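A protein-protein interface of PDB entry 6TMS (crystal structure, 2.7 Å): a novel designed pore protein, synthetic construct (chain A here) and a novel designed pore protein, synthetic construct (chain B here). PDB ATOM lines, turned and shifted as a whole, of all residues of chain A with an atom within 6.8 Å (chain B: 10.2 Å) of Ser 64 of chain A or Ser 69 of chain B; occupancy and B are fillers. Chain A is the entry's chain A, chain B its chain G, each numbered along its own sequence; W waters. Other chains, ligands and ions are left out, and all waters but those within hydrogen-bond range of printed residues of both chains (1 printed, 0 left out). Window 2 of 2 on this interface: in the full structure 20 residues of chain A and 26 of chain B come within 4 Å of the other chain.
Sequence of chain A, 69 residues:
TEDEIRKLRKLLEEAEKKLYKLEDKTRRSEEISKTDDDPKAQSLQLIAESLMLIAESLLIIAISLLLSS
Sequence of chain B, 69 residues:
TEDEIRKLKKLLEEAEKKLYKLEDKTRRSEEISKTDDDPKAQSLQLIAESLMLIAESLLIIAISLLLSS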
ATOM      1  N   LEU A  12      32.973   1.779  -7.553  1.00  0.00           N
ATOM      2  CA  LEU A  12      31.617   1.923  -8.038  1.00  0.00           C
ATOM      3  C   LEU A  12      31.603   2.269  -9.525  1.00  0.00           C
ATOM      4  O   LEU A  12      30.897   1.646 -10.337  1.00  0.00           O
ATOM      5  CB  LEU A  12      30.978   3.032  -7.225  1.00  0.00           C
ATOM      6  CG  LEU A  12      29.479   3.188  -7.232  1.00  0.00           C
ATOM      7  CD1 LEU A  12      29.211   4.550  -6.581  1.00  0.00           C
ATOM      8  CD2 LEU A  12      28.890   3.027  -8.648  1.00  0.00           C
ATOM      9  N   LEU A  59      23.472  -1.433  -9.483  1.00  0.00           N
ATOM     10  CA  LEU A  59      24.560  -0.496  -9.605  1.00  0.00           C
ATOM     11  C   LEU A  59      24.070   0.896  -9.268  1.00  0.00           C
ATOM     12  O   LEU A  59      24.717   1.635  -8.522  1.00  0.00           O
ATOM     13  CB  LEU A  59      25.078  -0.575 -11.029  1.00  0.00           C
ATOM     14  CG  LEU A  59      26.516  -1.029 -11.229  1.00  0.00           C
ATOM     15  CD1 LEU A  59      26.688  -1.519 -12.628  1.00  0.00           C
ATOM     16  CD2 LEU A  59      27.484   0.098 -10.996  1.00  0.00           C
ATOM     17  N   ILE A  60      22.889   1.251  -9.751  1.00  0.00           N
ATOM     18  CA  ILE A  60      22.420   2.593  -9.461  1.00  0.00           C
ATOM     19  C   ILE A  60      22.109   2.748  -7.959  1.00  0.00           C
ATOM     20  O   ILE A  60      22.295   3.824  -7.378  1.00  0.00           O
ATOM     21  CB  ILE A  60      21.210   2.912 -10.357  1.00  0.00           C
ATOM     22  CG1 ILE A  60      21.365   2.543 -11.874  1.00  0.00           C
ATOM     23  CG2 ILE A  60      20.924   4.289 -10.276  1.00  0.00           C
ATOM     24  CD1 ILE A  60      22.373   3.238 -12.799  1.00  0.00           C
ATOM     25  N   ILE A  61      21.590   1.702  -7.308  1.00  0.00           N
ATOM     26  CA  ILE A  61      21.341   1.800  -5.864  1.00  0.00           C
ATOM     27  C   ILE A  61      22.657   1.857  -5.139  1.00  0.00           C
ATOM     28  O   ILE A  61      22.806   2.547  -4.129  1.00  0.00           O
ATOM     29  CB  ILE A  61      20.462   0.625  -5.375  1.00  0.00           C
ATOM     30  CG1 ILE A  61      19.035   0.789  -5.895  1.00  0.00           C
ATOM     31  CG2 ILE A  61      20.407   0.493  -3.807  1.00  0.00           C
ATOM     32  CD1 ILE A  61      18.347  -0.472  -6.246  1.00  0.00           C
ATOM     33  N   ALA A  62      23.648   1.165  -5.648  1.00  0.00           N
ATOM     34  CA  ALA A  62      24.922   1.283  -5.000  1.00  0.00           C
ATOM     35  C   ALA A  62      25.404   2.730  -5.090  1.00  0.00           C
ATOM     36  O   ALA A  62      25.823   3.304  -4.075  1.00  0.00           O
ATOM     37  CB  ALA A  62      25.885   0.272  -5.607  1.00  0.00           C
ATOM     38  N   ILE A  63      25.257   3.395  -6.248  1.00  0.00           N
ATOM     39  CA  ILE A  63      25.691   4.796  -6.265  1.00  0.00           C
ATOM     40  C   ILE A  63      24.885   5.603  -5.249  1.00  0.00           C
ATOM     41  O   ILE A  63      25.447   6.338  -4.425  1.00  0.00           O
ATOM     42  CB  ILE A  63      25.631   5.450  -7.664  1.00  0.00           C
ATOM     43  CG1 ILE A  63      25.844   4.487  -8.838  1.00  0.00           C
ATOM     44  CG2 ILE A  63      26.785   6.539  -7.738  1.00  0.00           C
ATOM     45  CD1 ILE A  63      25.476   5.101 -10.194  1.00  0.00           C
ATOM     46  N   SER A  64      23.566   5.457  -5.246  1.00  0.00           N
ATOM     47  CA  SER A  64      22.838   6.376  -4.384  1.00  0.00           C
ATOM     48  C   SER A  64      23.124   6.098  -2.924  1.00  0.00           C
ATOM     49  O   SER A  64      23.233   7.030  -2.134  1.00  0.00           O
ATOM     50  CB  SER A  64      21.340   6.317  -4.633  1.00  0.00           C
ATOM     51  OG  SER A  64      20.647   7.141  -3.700  1.00  0.00           O
ATOM     52  N   LEU A  65      23.280   4.842  -2.533  1.00  0.00           N
ATOM     53  CA  LEU A  65      23.504   4.615  -1.115  1.00  0.00           C
ATOM     54  C   LEU A  65      24.867   5.119  -0.718  1.00  0.00           C
ATOM     55  O   LEU A  65      25.050   5.627   0.395  1.00  0.00           O
ATOM     56  CB  LEU A  65      23.384   3.141  -0.742  1.00  0.00           C
ATOM     57  CG  LEU A  65      21.933   2.656  -0.507  1.00  0.00           C
ATOM     58  CD1 LEU A  65      21.872   1.206  -0.063  1.00  0.00           C
ATOM     59  CD2 LEU A  65      21.071   3.519   0.427  1.00  0.00           C
ATOM     60  N   LEU A  66      25.823   5.043  -1.631  1.00  0.00           N
ATOM     61  CA  LEU A  66      27.128   5.556  -1.275  1.00  0.00           C
ATOM     62  C   LEU A  66      27.087   7.054  -1.053  1.00  0.00           C
ATOM     63  O   LEU A  66      27.583   7.556  -0.039  1.00  0.00           O
ATOM     64  CB  LEU A  66      28.120   5.206  -2.380  1.00  0.00           C
ATOM     65  CG  LEU A  66      29.531   5.782  -2.192  1.00  0.00           C
ATOM     66  CD1 LEU A  66      30.204   5.320  -0.922  1.00  0.00           C
ATOM     67  CD2 LEU A  66      30.418   5.386  -3.374  1.00  0.00           C
ATOM     68  N   LEU A  67      26.416   7.775  -1.923  1.00  0.00           N
ATOM     69  CA  LEU A  67      26.354   9.202  -1.689  1.00  0.00           C
ATOM     70  C   LEU A  67      25.384   9.540  -0.573  1.00  0.00           C
ATOM     71  O   LEU A  67      25.454  10.625   0.005  1.00  0.00           O
ATOM     72  CB  LEU A  67      26.001   9.895  -2.992  1.00  0.00           C
ATOM     73  CG  LEU A  67      27.071   9.682  -4.089  1.00  0.00           C
ATOM     74  CD1 LEU A  67      26.577  10.187  -5.441  1.00  0.00           C
ATOM     75  CD2 LEU A  67      28.455  10.289  -3.792  1.00  0.00           C
ATOM     76  N   SER A  68      24.492   8.629  -0.240  1.00  0.00           N
ATOM     77  CA  SER A  68      23.517   8.958   0.768  1.00  0.00           C
ATOM     78  C   SER A  68      24.154   8.988   2.134  1.00  0.00           C
ATOM     79  O   SER A  68      23.548   9.489   3.082  1.00  0.00           O
ATOM     80  CB  SER A  68      22.394   7.942   0.735  1.00  0.00           C
ATOM     81  OG  SER A  68      21.544   8.135   1.842  1.00  0.00           O
ATOM     82  N   SER A  69      25.365   8.483   2.240  1.00  0.00           N
ATOM     83  CA  SER A  69      26.138   8.626   3.436  1.00  0.00           C
ATOM     84  C   SER A  69      26.438  10.106   3.670  1.00  0.00           C
ATOM     85  O   SER A  69      25.889  10.723   4.586  1.00  0.00           O
ATOM     86  CB  SER A  69      27.399   7.805   3.283  1.00  0.00           C
ATOM     87  OG  SER A  69      28.157   8.334   2.211  1.00  0.00           O
ATOM     88  N   THR B   1      26.331  17.823  -7.395  1.00  0.00           N
ATOM     89  CA  THR B   1      25.245  17.264  -6.595  1.00  0.00           C
ATOM     90  C   THR B   1      24.012  17.584  -7.382  1.00  0.00           C
ATOM     91  O   THR B   1      23.034  16.860  -7.358  1.00  0.00           O
ATOM     92  CB  THR B   1      25.193  17.864  -5.204  1.00  0.00           C
ATOM     93  OG1 THR B   1      24.488  16.975  -4.353  1.00  0.00           O
ATOM     94  CG2 THR B   1      24.485  19.206  -5.176  1.00  0.00           C
ATOM     95  N   GLU B   4      24.951  15.647 -10.439  1.00  0.00           N
ATOM     96  CA  GLU B   4      25.097  14.250 -10.084  1.00  0.00           C
ATOM     97  C   GLU B   4      23.769  13.493 -10.122  1.00  0.00           C
ATOM     98  O   GLU B   4      23.677  12.450 -10.780  1.00  0.00           O
ATOM     99  CB  GLU B   4      25.769  14.156  -8.720  1.00  0.00           C
ATOM    100  CG  GLU B   4      26.064  12.744  -8.268  1.00  0.00           C
ATOM    101  CD  GLU B   4      26.633  11.821  -9.361  1.00  0.00           C
ATOM    102  OE1 GLU B   4      26.046  11.751 -10.459  1.00  0.00           O
ATOM    103  OE2 GLU B   4      27.644  11.120  -9.111  1.00  0.00           O
ATOM    104  N   ILE B   5      22.709  14.007  -9.496  1.00  0.00           N
ATOM    105  CA  ILE B   5      21.457  13.255  -9.607  1.00  0.00           C
ATOM    106  C   ILE B   5      20.864  13.354 -11.007  1.00  0.00           C
ATOM    107  O   ILE B   5      19.981  12.555 -11.335  1.00  0.00           O
ATOM    108  CB  ILE B   5      20.407  13.594  -8.525  1.00  0.00           C
ATOM    109  CG1 ILE B   5      20.684  12.767  -7.255  1.00  0.00           C
ATOM    110  CG2 ILE B   5      18.977  13.227  -8.974  1.00  0.00           C
ATOM    111  CD1 ILE B   5      19.777  13.087  -6.013  1.00  0.00           C
ATOM    112  N   LYS B   7      22.619  12.867 -13.746  1.00  0.00           N
ATOM    113  CA  LYS B   7      23.266  11.734 -14.401  1.00  0.00           C
ATOM    114  C   LYS B   7      22.759  10.438 -13.817  1.00  0.00           C
ATOM    115  O   LYS B   7      22.607   9.434 -14.525  1.00  0.00           O
ATOM    116  CB  LYS B   7      24.786  11.869 -14.258  1.00  0.00           C
ATOM    117  CG  LYS B   7      25.674  10.928 -15.143  1.00  0.00           C
ATOM    118  CD  LYS B   7      25.543  11.179 -16.669  1.00  0.00           C
ATOM    119  CE  LYS B   7      26.084  10.034 -17.575  1.00  0.00           C
ATOM    120  NZ  LYS B   7      27.467   9.518 -17.311  1.00  0.00           N
ATOM    121  N   LEU B   8      22.455  10.456 -12.535  1.00  0.00           N
ATOM    122  CA  LEU B   8      21.760   9.321 -11.981  1.00  0.00           C
ATOM    123  C   LEU B   8      20.373   9.198 -12.625  1.00  0.00           C
ATOM    124  O   LEU B   8      19.962   8.108 -13.028  1.00  0.00           O
ATOM    125  CB  LEU B   8      21.716   9.467 -10.460  1.00  0.00           C
ATOM    126  CG  LEU B   8      21.045   8.318  -9.715  1.00  0.00           C
ATOM    127  CD1 LEU B   8      21.020   7.152 -10.604  1.00  0.00           C
ATOM    128  CD2 LEU B   8      21.703   7.910  -8.383  1.00  0.00           C
ATOM    129  N   LYS B   9      19.668  10.304 -12.793  1.00  0.00           N
ATOM    130  CA  LYS B   9      18.367  10.260 -13.450  1.00  0.00           C
ATOM    131  C   LYS B   9      18.510   9.751 -14.875  1.00  0.00           C
ATOM    132  O   LYS B   9      17.654   9.028 -15.378  1.00  0.00           O
ATOM    133  CB  LYS B   9      17.746  11.657 -13.432  1.00  0.00           C
ATOM    134  CG  LYS B   9      16.214  11.718 -13.389  1.00  0.00           C
ATOM    135  CD  LYS B   9      15.743  13.045 -12.734  1.00  0.00           C
ATOM    136  CE  LYS B   9      14.402  13.594 -13.254  1.00  0.00           C
ATOM    137  NZ  LYS B   9      13.264  12.699 -13.008  1.00  0.00           N
ATOM    138  N   LEU B  11      20.735   7.648 -15.990  1.00  0.00           N
ATOM    139  CA  LEU B  11      20.907   6.217 -15.887  1.00  0.00           C
ATOM    140  C   LEU B  11      19.595   5.534 -15.583  1.00  0.00           C
ATOM    141  O   LEU B  11      19.241   4.520 -16.192  1.00  0.00           O
ATOM    142  CB  LEU B  11      21.909   5.960 -14.777  1.00  0.00           C
ATOM    143  CG  LEU B  11      23.317   6.382 -15.171  1.00  0.00           C
ATOM    144  CD1 LEU B  11      24.271   6.339 -13.975  1.00  0.00           C
ATOM    145  CD2 LEU B  11      23.794   5.503 -16.325  1.00  0.00           C
ATOM    146  N   LEU B  12      18.840   6.136 -14.682  1.00  0.00           N
ATOM    147  CA  LEU B  12      17.595   5.570 -14.199  1.00  0.00           C
ATOM    148  C   LEU B  12      16.526   5.580 -15.292  1.00  0.00           C
ATOM    149  O   LEU B  12      15.751   4.624 -15.432  1.00  0.00           O
ATOM    150  CB  LEU B  12      17.189   6.369 -12.952  1.00  0.00           C
ATOM    151  CG  LEU B  12      16.670   5.715 -11.642  1.00  0.00           C
ATOM    152  CD1 LEU B  12      17.215   4.297 -11.353  1.00  0.00           C
ATOM    153  CD2 LEU B  12      16.938   6.607 -10.402  1.00  0.00           C
ATOM    154  N   LEU B  58      13.277  -3.492  -8.643  1.00  0.00           N
ATOM    155  CA  LEU B  58      14.553  -2.890  -8.307  1.00  0.00           C
ATOM    156  C   LEU B  58      14.693  -1.542  -8.960  1.00  0.00           C
ATOM    157  O   LEU B  58      15.188  -0.589  -8.358  1.00  0.00           O
ATOM    158  CB  LEU B  58      15.662  -3.830  -8.734  1.00  0.00           C
ATOM    159  CG  LEU B  58      15.965  -4.871  -7.658  1.00  0.00           C
ATOM    160  CD1 LEU B  58      17.113  -5.626  -8.101  1.00  0.00           C
ATOM    161  CD2 LEU B  58      16.308  -4.273  -6.277  1.00  0.00           C
ATOM    162  N   LEU B  59      14.149  -1.412 -10.143  1.00  0.00           N
ATOM    163  CA  LEU B  59      14.146  -0.116 -10.761  1.00  0.00           C
ATOM    164  C   LEU B  59      13.320   0.845  -9.936  1.00  0.00           C
ATOM    165  O   LEU B  59      13.697   2.002  -9.749  1.00  0.00           O
ATOM    166  CB  LEU B  59      13.575  -0.266 -12.151  1.00  0.00           C
ATOM    167  CG  LEU B  59      13.963   0.573 -13.350  1.00  0.00           C
ATOM    168  CD1 LEU B  59      13.084   0.092 -14.511  1.00  0.00           C
ATOM    169  CD2 LEU B  59      13.743   2.046 -13.103  1.00  0.00           C
ATOM    170  N   ILE B  60      12.183   0.386  -9.426  1.00  0.00           N
ATOM    171  CA  ILE B  60      11.389   1.294  -8.620  1.00  0.00           C
ATOM    172  C   ILE B  60      12.124   1.633  -7.339  1.00  0.00           C
ATOM    173  O   ILE B  60      12.034   2.755  -6.843  1.00  0.00           O
ATOM    174  CB  ILE B  60       9.983   0.708  -8.389  1.00  0.00           C
ATOM    175  CG1 ILE B  60       9.033   0.967  -9.580  1.00  0.00           C
ATOM    176  CG2 ILE B  60       9.332   1.313  -7.176  1.00  0.00           C
ATOM    177  CD1 ILE B  60       9.565   0.724 -10.983  1.00  0.00           C
ATOM    178  N   ILE B  61      12.872   0.702  -6.776  1.00  0.00           N
ATOM    179  CA  ILE B  61      13.618   1.060  -5.586  1.00  0.00           C
ATOM    180  C   ILE B  61      14.679   2.082  -5.923  1.00  0.00           C
ATOM    181  O   ILE B  61      14.939   3.001  -5.150  1.00  0.00           O
ATOM    182  CB  ILE B  61      14.207  -0.207  -4.955  1.00  0.00           C
ATOM    183  CG1 ILE B  61      13.080  -0.997  -4.285  1.00  0.00           C
ATOM    184  CG2 ILE B  61      15.336   0.129  -3.993  1.00  0.00           C
ATOM    185  CD1 ILE B  61      13.295  -2.479  -4.199  1.00  0.00           C
ATOM    186  N   ALA B  62      15.292   1.975  -7.080  1.00  0.00           N
ATOM    187  CA  ALA B  62      16.273   2.992  -7.393  1.00  0.00           C
ATOM    188  C   ALA B  62      15.593   4.338  -7.588  1.00  0.00           C
ATOM    189  O   ALA B  62      16.044   5.359  -7.059  1.00  0.00           O
ATOM    190  CB  ALA B  62      17.078   2.567  -8.608  1.00  0.00           C
ATOM    191  N   ILE B  63      14.463   4.358  -8.283  1.00  0.00           N
ATOM    192  CA  ILE B  63      13.771   5.622  -8.467  1.00  0.00           C
ATOM    193  C   ILE B  63      13.477   6.233  -7.103  1.00  0.00           C
ATOM    194  O   ILE B  63      13.693   7.424  -6.863  1.00  0.00           O
ATOM    195  CB  ILE B  63      12.483   5.404  -9.283  1.00  0.00           C
ATOM    196  CG1 ILE B  63      12.769   4.821 -10.683  1.00  0.00           C
ATOM    197  CG2 ILE B  63      11.748   6.733  -9.454  1.00  0.00           C
ATOM    198  CD1 ILE B  63      11.550   4.116 -11.322  1.00  0.00           C
ATOM    199  N   SER B  64      12.965   5.417  -6.195  1.00  0.00           N
ATOM    200  CA  SER B  64      12.486   5.923  -4.919  1.00  0.00           C
ATOM    201  C   SER B  64      13.614   6.261  -3.966  1.00  0.00           C
ATOM    202  O   SER B  64      13.450   7.103  -3.084  1.00  0.00           O
ATOM    203  CB  SER B  64      11.516   4.931  -4.308  1.00  0.00           C
ATOM    204  OG  SER B  64      10.255   5.561  -4.188  1.00  0.00           O
ATOM    205  N   LEU B  65      14.713   5.544  -4.040  1.00  0.00           N
ATOM    206  CA  LEU B  65      15.844   5.913  -3.220  1.00  0.00           C
ATOM    207  C   LEU B  65      16.407   7.211  -3.705  1.00  0.00           C
ATOM    208  O   LEU B  65      16.875   8.041  -2.923  1.00  0.00           O
ATOM    209  CB  LEU B  65      16.893   4.819  -3.283  1.00  0.00           C
ATOM    210  CG  LEU B  65      16.748   3.820  -2.145  1.00  0.00           C
ATOM    211  CD1 LEU B  65      17.366   2.503  -2.430  1.00  0.00           C
ATOM    212  CD2 LEU B  65      17.493   4.422  -0.966  1.00  0.00           C
ATOM    213  N   LEU B  66      16.331   7.423  -4.994  1.00  0.00           N
ATOM    214  CA  LEU B  66      16.815   8.683  -5.473  1.00  0.00           C
ATOM    215  C   LEU B  66      15.871   9.776  -5.036  1.00  0.00           C
ATOM    216  O   LEU B  66      16.303  10.878  -4.697  1.00  0.00           O
ATOM    217  CB  LEU B  66      16.956   8.593  -6.979  1.00  0.00           C
ATOM    218  CG  LEU B  66      17.762   9.716  -7.595  1.00  0.00           C
ATOM    219  CD1 LEU B  66      19.125   9.666  -6.931  1.00  0.00           C
ATOM    220  CD2 LEU B  66      17.933   9.486  -9.102  1.00  0.00           C
ATOM    221  N   LEU B  67      14.597   9.445  -4.933  1.00  0.00           N
ATOM    222  CA  LEU B  67      13.624  10.410  -4.464  1.00  0.00           C
ATOM    223  C   LEU B  67      13.799  10.684  -2.984  1.00  0.00           C
ATOM    224  O   LEU B  67      13.466  11.768  -2.493  1.00  0.00           O
ATOM    225  CB  LEU B  67      12.250   9.845  -4.766  1.00  0.00           C
ATOM    226  CG  LEU B  67      11.026  10.578  -4.276  1.00  0.00           C
ATOM    227  CD1 LEU B  67      10.340  11.243  -5.455  1.00  0.00           C
ATOM    228  CD2 LEU B  67      10.125   9.589  -3.628  1.00  0.00           C
ATOM    229  N   SER B  68      14.355   9.728  -2.278  1.00  0.00           N
ATOM    230  CA  SER B  68      14.565   9.838  -0.856  1.00  0.00           C
ATOM    231  C   SER B  68      15.805  10.619  -0.485  1.00  0.00           C
ATOM    232  O   SER B  68      15.938  11.028   0.669  1.00  0.00           O
ATOM    233  CB  SER B  68      14.680   8.437  -0.300  1.00  0.00           C
ATOM    234  OG  SER B  68      15.331   8.477   0.942  1.00  0.00           O
ATOM    235  N   SER B  69      16.694  10.856  -1.428  1.00  0.00           N
ATOM    236  CA  SER B  69      17.907  11.592  -1.156  1.00  0.00           C
ATOM    237  C   SER B  69      18.077  12.713  -2.139  1.00  0.00           C
ATOM    238  O   SER B  69      17.165  13.506  -2.307  1.00  0.00           O
ATOM    239  CB  SER B  69      19.091  10.643  -1.201  1.00  0.00           C
ATOM    240  OG  SER B  69      19.285  10.157  -2.512  1.00  0.00           O
HETATM  241  O   HOH W   1      19.338   4.939  -6.404  1.00  0.00           O
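The backbone carbonyl oxygen of Leu 65 of chain B lies within hydrogen-bond range of the side-chain hydroxyl of Ser 69 of chain B.
Water W1 bridges O of Ile 60 of chain A (3.3 Å) and O of Ala 62 of chain B (3.4 Å).
No residue of chain B comes within 4 Å of Ala 62 of chain A. No residue of chain B comes within 4 Å of Ile 63 of chain A. Ser 64 of chain A touches just these residues of chain B: Leu 65 and Ser 69. Leu 65 of chain A touches one residue of chain B. No residue of chain B comes within 4 Å of Ser 68 of chain A. Of the printed residues of chain A, Glu 4 of chain B touches Leu 67 (3.8 Å). Lys 7 of chain B touches none of the printed residues of chain A. Printed residues of chain A within 4 Å of Leu 8 of chain B: Ile 60. Printed residues of chain A within 4 Å of Leu 11 of chain B: Ile 60 (3.4 Å). Of the printed residues of chain A, Leu 58 of chain B touches Ile 61 (3.8 Å). Leu 59 of chain B touches none of the printed residues of chain A. Of the printed residues of chain A, Ala 62 of chain B touches Ile 61 (3.8 Å). The nearest residue of chain A that does not touch Ser 69 of chain B is Ser 68 of chain A (4.6 Å).
Ile 60 of chain A touches Leu 8 of chain B (CG2 to CD1, 2.9 Å). Ile 60 of chain A touches Leu 11 of chain B. Ile 60 of chain A touches Leu 12 of chain B. O of Leu 58 of chain B touches CD1 of Ile 61 of chain A, 3.8 Å away. Ile 61 of chain A touches Ile 61 of chain B. Ile 61 of chain A touches Ala 62 of chain B. Leu 65 of chain B touches Ile 61 of chain A. OG of Ser 64 of chain A touches OG of Ser 69 of chain B, 3.5 Å away. Leu 65 of chain A touches Leu 65 of chain B (CD2 to CD2, 3.9 Å). Leu 67 of chain A touches Glu 4 of chain B.
Of the 20 printed residues of chain B, 9 touch a printed residue of chain A. Printed residues of chain B that touch a printed residue of chain A: Glu 4, Leu 8, Leu 11, Leu 12, Leu 58, Ile 61, Ala 62, Leu 65 and Ser 69. Of the 12 printed residues of chain A, 5 touch a printed residue of chain B. Printed residues of chain A that touch a printed residue of chain B: Ile 60, Ile 61, Ser 64, Leu 65 and Leu 67. Among the printed residues, no Asp or Glu carboxylate lies within 4 Å of a Lys or Arg side-chain nitrogen of the other chain.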
